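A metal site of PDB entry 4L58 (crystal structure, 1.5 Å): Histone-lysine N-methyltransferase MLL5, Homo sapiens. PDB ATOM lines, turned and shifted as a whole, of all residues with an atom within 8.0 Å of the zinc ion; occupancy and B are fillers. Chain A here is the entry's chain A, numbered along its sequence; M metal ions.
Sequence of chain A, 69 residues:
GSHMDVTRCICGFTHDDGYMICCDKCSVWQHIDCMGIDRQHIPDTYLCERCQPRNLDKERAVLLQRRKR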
ATOM      1  N   ARG A   8     -16.048  -6.737 -14.000  1.00  0.00           N
ATOM      2  CA  ARG A   8     -15.109  -5.682 -14.384  1.00  0.00           C
ATOM      3  C   ARG A   8     -15.585  -5.060 -15.688  1.00  0.00           C
ATOM      4  O   ARG A   8     -15.298  -5.559 -16.770  1.00  0.00           O
ATOM      5  CB  ARG A   8     -13.686  -6.199 -14.569  1.00  0.00           C
ATOM      6  CG  ARG A   8     -12.676  -5.073 -14.767  1.00  0.00           C
ATOM      7  CD  ARG A   8     -11.362  -5.543 -15.380  1.00  0.00           C
ATOM      8  NE  ARG A   8     -11.552  -6.079 -16.722  1.00  0.00           N
ATOM      9  CZ  ARG A   8     -11.846  -5.343 -17.786  1.00  0.00           C
ATOM     10  NH1 ARG A   8     -11.983  -4.022 -17.689  1.00  0.00           N
ATOM     11  NH2 ARG A   8     -12.003  -5.928 -18.967  1.00  0.00           N
ATOM     12  N   CYS A  22     -20.547 -12.097 -20.247  1.00  0.00           N
ATOM     13  CA  CYS A  22     -19.332 -12.640 -19.670  1.00  0.00           C
ATOM     14  C   CYS A  22     -18.260 -12.858 -20.726  1.00  0.00           C
ATOM     15  O   CYS A  22     -18.528 -13.454 -21.779  1.00  0.00           O
ATOM     16  CB  CYS A  22     -19.654 -13.975 -18.979  1.00  0.00           C
ATOM     17  SG  CYS A  22     -18.306 -14.671 -18.010  1.00  0.00           S
ATOM     18  N   CYS A  23     -17.043 -12.389 -20.454  1.00  0.00           N
ATOM     19  CA  CYS A  23     -15.928 -12.579 -21.376  1.00  0.00           C
ATOM     20  C   CYS A  23     -15.556 -14.052 -21.485  1.00  0.00           C
ATOM     21  O   CYS A  23     -15.298 -14.718 -20.484  1.00  0.00           O
ATOM     22  CB  CYS A  23     -14.708 -11.786 -20.931  1.00  0.00           C
ATOM     23  SG  CYS A  23     -13.296 -11.949 -22.063  1.00  0.00           S
ATOM     24  N   ASP A  24     -15.519 -14.555 -22.721  1.00  0.00           N
ATOM     25  CA  ASP A  24     -15.250 -15.957 -22.957  1.00  0.00           C
ATOM     26  C   ASP A  24     -13.813 -16.340 -22.625  1.00  0.00           C
ATOM     27  O   ASP A  24     -13.520 -17.522 -22.403  1.00  0.00           O
ATOM     28  CB  ASP A  24     -15.587 -16.324 -24.392  1.00  0.00           C
ATOM     29  CG  ASP A  24     -17.087 -16.474 -24.603  1.00  0.00           C
ATOM     30  OD1 ASP A  24     -17.759 -16.970 -23.679  1.00  0.00           O
ATOM     31  OD2 ASP A  24     -17.582 -16.097 -25.678  1.00  0.00           O
ATOM     32  N   LYS A  25     -12.914 -15.366 -22.580  1.00  0.00           N
ATOM     33  CA  LYS A  25     -11.529 -15.645 -22.236  1.00  0.00           C
ATOM     34  C   LYS A  25     -11.260 -15.502 -20.739  1.00  0.00           C
ATOM     35  O   LYS A  25     -10.828 -16.453 -20.092  1.00  0.00           O
ATOM     36  CB  LYS A  25     -10.589 -14.742 -23.032  1.00  0.00           C
ATOM     37  CG  LYS A  25      -9.121 -14.897 -22.663  1.00  0.00           C
ATOM     38  CD  LYS A  25      -8.243 -14.123 -23.602  1.00  0.00           C
ATOM     39  CE  LYS A  25      -6.862 -13.883 -23.021  1.00  0.00           C
ATOM     40  NZ  LYS A  25      -5.919 -13.519 -24.107  1.00  0.00           N
ATOM     41  N   CYS A  26     -11.531 -14.320 -20.186  1.00  0.00           N
ATOM     42  CA  CYS A  26     -11.122 -14.028 -18.803  1.00  0.00           C
ATOM     43  C   CYS A  26     -12.250 -14.131 -17.781  1.00  0.00           C
ATOM     44  O   CYS A  26     -12.017 -14.053 -16.578  1.00  0.00           O
ATOM     45  CB  CYS A  26     -10.468 -12.647 -18.731  1.00  0.00           C
ATOM     46  SG  CYS A  26     -11.634 -11.275 -18.822  1.00  0.00           S
ATOM     47  N   SER A  27     -13.481 -14.302 -18.268  1.00  0.00           N
ATOM     48  CA  SER A  27     -14.656 -14.565 -17.429  1.00  0.00           C
ATOM     49  C   SER A  27     -15.184 -13.380 -16.613  1.00  0.00           C
ATOM     50  O   SER A  27     -16.064 -13.582 -15.764  1.00  0.00           O
ATOM     51  CB  SER A  27     -14.413 -15.752 -16.501  1.00  0.00           C
ATOM     52  OG  SER A  27     -14.184 -16.937 -17.237  1.00  0.00           O
ATOM     53  N   VAL A  28     -14.696 -12.174 -16.843  1.00  0.00           N
ATOM     54  CA  VAL A  28     -15.294 -11.027 -16.155  1.00  0.00           C
ATOM     55  C   VAL A  28     -16.648 -10.704 -16.771  1.00  0.00           C
ATOM     56  O   VAL A  28     -16.883 -10.949 -17.963  1.00  0.00           O
ATOM     57  CB  VAL A  28     -14.418  -9.747 -16.165  1.00  0.00           C
ATOM     58  CG1 VAL A  28     -13.066 -10.029 -15.536  1.00  0.00           C
ATOM     59  CG2 VAL A  28     -14.280  -9.171 -17.567  1.00  0.00           C
ATOM     60  N   TRP A  29     -17.522 -10.154 -15.946  1.00  0.00           N
ATOM     61  CA  TRP A  29     -18.849  -9.759 -16.384  1.00  0.00           C
ATOM     62  C   TRP A  29     -18.883  -8.263 -16.630  1.00  0.00           C
ATOM     63  O   TRP A  29     -18.266  -7.490 -15.896  1.00  0.00           O
ATOM     64  CB  TRP A  29     -19.887 -10.120 -15.329  1.00  0.00           C
ATOM     65  CG  TRP A  29     -20.122 -11.582 -15.221  1.00  0.00           C
ATOM     66  CD1 TRP A  29     -19.440 -12.462 -14.444  1.00  0.00           C
ATOM     67  CD2 TRP A  29     -21.109 -12.331 -15.923  1.00  0.00           C
ATOM     68  NE1 TRP A  29     -19.949 -13.727 -14.615  1.00  0.00           N
ATOM     69  CE2 TRP A  29     -20.978 -13.677 -15.521  1.00  0.00           C
ATOM     70  CE3 TRP A  29     -22.094 -12.006 -16.863  1.00  0.00           C
ATOM     71  CZ2 TRP A  29     -21.783 -14.689 -16.010  1.00  0.00           C
ATOM     72  CZ3 TRP A  29     -22.900 -13.005 -17.348  1.00  0.00           C
ATOM     73  CH2 TRP A  29     -22.744 -14.340 -16.931  1.00  0.00           C
ATOM     74  N   GLN A  30     -19.614  -7.871 -17.659  1.00  0.00           N
ATOM     75  CA  GLN A  30     -19.723  -6.473 -18.033  1.00  0.00           C
ATOM     76  C   GLN A  30     -21.171  -6.169 -18.351  1.00  0.00           C
ATOM     77  O   GLN A  30     -21.945  -7.066 -18.681  1.00  0.00           O
ATOM     78  CB  GLN A  30     -18.832  -6.185 -19.240  1.00  0.00           C
ATOM     79  CG  GLN A  30     -17.424  -6.754 -19.103  1.00  0.00           C
ATOM     80  CD  GLN A  30     -16.475  -6.183 -20.114  1.00  0.00           C
ATOM     81  OE1 GLN A  30     -16.605  -6.426 -21.315  1.00  0.00           O
ATOM     82  NE2 GLN A  30     -15.519  -5.376 -19.650  1.00  0.00           N
ATOM     83  N   TYR A  46     -18.031 -13.668 -27.067  1.00  0.00           N
ATOM     84  CA  TYR A  46     -17.821 -12.310 -26.574  1.00  0.00           C
ATOM     85  C   TYR A  46     -16.513 -12.191 -25.814  1.00  0.00           C
ATOM     86  O   TYR A  46     -16.229 -12.997 -24.931  1.00  0.00           O
ATOM     87  CB  TYR A  46     -18.964 -11.856 -25.666  1.00  0.00           C
ATOM     88  CG  TYR A  46     -18.682 -10.490 -25.090  1.00  0.00           C
ATOM     89  CD1 TYR A  46     -18.901  -9.344 -25.836  1.00  0.00           C
ATOM     90  CD2 TYR A  46     -18.157 -10.333 -23.816  1.00  0.00           C
ATOM     91  CE1 TYR A  46     -18.630  -8.094 -25.341  1.00  0.00           C
ATOM     92  CE2 TYR A  46     -17.878  -9.073 -23.302  1.00  0.00           C
ATOM     93  CZ  TYR A  46     -18.127  -7.959 -24.073  1.00  0.00           C
ATOM     94  OH  TYR A  46     -17.855  -6.695 -23.596  1.00  0.00           O
ATOM     95  N   LEU A  47     -15.728 -11.185 -26.171  1.00  0.00           N
ATOM     96  CA  LEU A  47     -14.506 -10.859 -25.426  1.00  0.00           C
ATOM     97  C   LEU A  47     -14.589  -9.431 -24.907  1.00  0.00           C
ATOM     98  O   LEU A  47     -15.074  -8.533 -25.585  1.00  0.00           O
ATOM     99  CB  LEU A  47     -13.275 -10.992 -26.319  1.00  0.00           C
ATOM    100  CG  LEU A  47     -12.973 -12.380 -26.871  1.00  0.00           C
ATOM    101  CD1 LEU A  47     -11.746 -12.321 -27.758  1.00  0.00           C
ATOM    102  CD2 LEU A  47     -12.763 -13.370 -25.729  1.00  0.00           C
ATOM    103  N   CYS A  48     -14.095  -9.240 -23.681  1.00  0.00           N
ATOM    104  CA  CYS A  48     -14.048  -7.902 -23.087  1.00  0.00           C
ATOM    105  C   CYS A  48     -13.035  -7.021 -23.821  1.00  0.00           C
ATOM    106  O   CYS A  48     -12.337  -7.470 -24.740  1.00  0.00           O
ATOM    107  CB  CYS A  48     -13.706  -7.982 -21.598  1.00  0.00           C
ATOM    108  SG  CYS A  48     -11.975  -8.358 -21.230  1.00  0.00           S
ATOM    109  N   GLU A  49     -12.955  -5.766 -23.403  1.00  0.00           N
ATOM    110  CA  GLU A  49     -12.153  -4.779 -24.117  1.00  0.00           C
ATOM    111  C   GLU A  49     -10.660  -4.886 -23.778  1.00  0.00           C
ATOM    112  O   GLU A  49      -9.842  -4.190 -24.368  1.00  0.00           O
ATOM    113  CB  GLU A  49     -12.687  -3.364 -23.861  1.00  0.00           C
ATOM    114  CG  GLU A  49     -12.158  -2.653 -22.623  1.00  0.00           C
ATOM    115  CD  GLU A  49     -12.531  -3.324 -21.318  1.00  0.00           C
ATOM    116  OE1 GLU A  49     -13.331  -4.283 -21.322  1.00  0.00           O
ATOM    117  OE2 GLU A  49     -12.023  -2.873 -20.272  1.00  0.00           O
ATOM    118  N   ARG A  50     -10.318  -5.756 -22.844  1.00  0.00           N
ATOM    119  CA  ARG A  50      -8.906  -6.061 -22.601  1.00  0.00           C
ATOM    120  C   ARG A  50      -8.472  -7.279 -23.402  1.00  0.00           C
ATOM    121  O   ARG A  50      -7.345  -7.319 -23.907  1.00  0.00           O
ATOM    122  CB  ARG A  50      -8.657  -6.314 -21.124  1.00  0.00           C
ATOM    123  CG  ARG A  50      -8.778  -5.084 -20.275  1.00  0.00           C
ATOM    124  CD  ARG A  50      -8.253  -5.375 -18.902  1.00  0.00           C
ATOM    125  NE  ARG A  50      -8.252  -4.194 -18.037  1.00  0.00           N
ATOM    126  CZ  ARG A  50      -7.943  -4.242 -16.749  1.00  0.00           C
ATOM    127  NH1 ARG A  50      -7.624  -5.392 -16.179  1.00  0.00           N
ATOM    128  NH2 ARG A  50      -7.957  -3.130 -16.019  1.00  0.00           N
ATOM    129  N   CYS A  51      -9.356  -8.258 -23.499  1.00  0.00           N
ATOM    130  CA  CYS A  51      -9.044  -9.486 -24.222  1.00  0.00           C
ATOM    131  C   CYS A  51      -9.138  -9.268 -25.720  1.00  0.00           C
ATOM    132  O   CYS A  51      -8.504  -9.973 -26.503  1.00  0.00           O
ATOM    133  CB  CYS A  51      -9.980 -10.614 -23.771  1.00  0.00           C
ATOM    134  SG  CYS A  51      -9.674 -11.179 -22.075  1.00  0.00           S
ATOM    135  N   GLN A  52      -9.934  -8.278 -26.118  1.00  0.00           N
ATOM    136  CA  GLN A  52     -10.029  -7.856 -27.510  1.00  0.00           C
ATOM    137  C   GLN A  52     -10.032  -6.334 -27.524  1.00  0.00           C
ATOM    138  O   GLN A  52     -11.093  -5.702 -27.558  1.00  0.00           O
ATOM    139  CB  GLN A  52     -11.313  -8.397 -28.152  1.00  0.00           C
ATOM    140  CG  GLN A  52     -11.491  -8.018 -29.610  1.00  0.00           C
ATOM    141  CD  GLN A  52     -12.933  -8.066 -30.037  1.00  0.00           C
ATOM    142  OE1 GLN A  52     -13.712  -8.901 -29.560  1.00  0.00           O
ATOM    143  NE2 GLN A  52     -13.320  -7.165 -30.935  1.00  0.00           N
ATOM    144  N   ARG A  54     -10.266  -2.533 -27.904  1.00  0.00           N
ATOM    145  CA  ARG A  54     -11.064  -1.688 -28.759  1.00  0.00           C
ATOM    146  C   ARG A  54     -11.471  -0.472 -27.946  1.00  0.00           C
ATOM    147  O   ARG A  54     -11.462  -0.507 -26.714  1.00  0.00           O
ATOM    148  CB  ARG A  54     -12.303  -2.436 -29.256  1.00  0.00           C
ATOM    149  CG  ARG A  54     -13.237  -2.914 -28.158  1.00  0.00           C
ATOM    150  CD  ARG A  54     -14.239  -3.902 -28.742  1.00  0.00           C
ATOM    151  NE  ARG A  54     -15.238  -4.372 -27.776  1.00  0.00           N
ATOM    152  CZ  ARG A  54     -15.065  -5.400 -26.942  1.00  0.00           C
ATOM    153  NH1 ARG A  54     -13.926  -6.072 -26.932  1.00  0.00           N
ATOM    154  NH2 ARG A  54     -16.050  -5.748 -26.125  1.00  0.00           N
HETATM  155 ZN    ZN M   1     -11.649 -10.676 -21.030  1.00  0.00          ZN
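Four residues have an atom within 4 Å of the zinc ion: Cys 23, Cys 26, Cys 48 and Cys 51.
The nearest printed residue that does not touch the zinc ion is Val 28 (4.6 Å).
N of Arg 50 lies close to SG of Cys 48 (3.5 Å).
The backbone carbonyl oxygen of Val 28 sits at hydrogen-bond distance from the backbone NH of Cys 23, at 2.9 Å.
NH1 of Arg 54 is in hydrogen-bond range of O of Cys 48, 3.0 Å away.
The side-chain sulfur (SG) of Cys 48 sits close to the guanidinium group (NH2) of Arg 8, at 3.3 Å.
SG of Cys 23 sits close to N of Lys 25 (3.5 Å).
The backbone NH (N) of Val 28 sits close to the side-chain sulfur (SG) of Cys 26 (3.8 Å).
SG of Cys 26 is bound to the zinc ion, at 2.3 Å.
SG of Cys 51 is bound to the zinc ion, at 2.3 Å.
The zinc ion is bound by SG of Cys 23, at 2.3 Å.
The side-chain sulfur (SG) of Cys 48 binds the zinc ion (2.3 Å).
The zinc ion has four donor atoms within binding distance.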
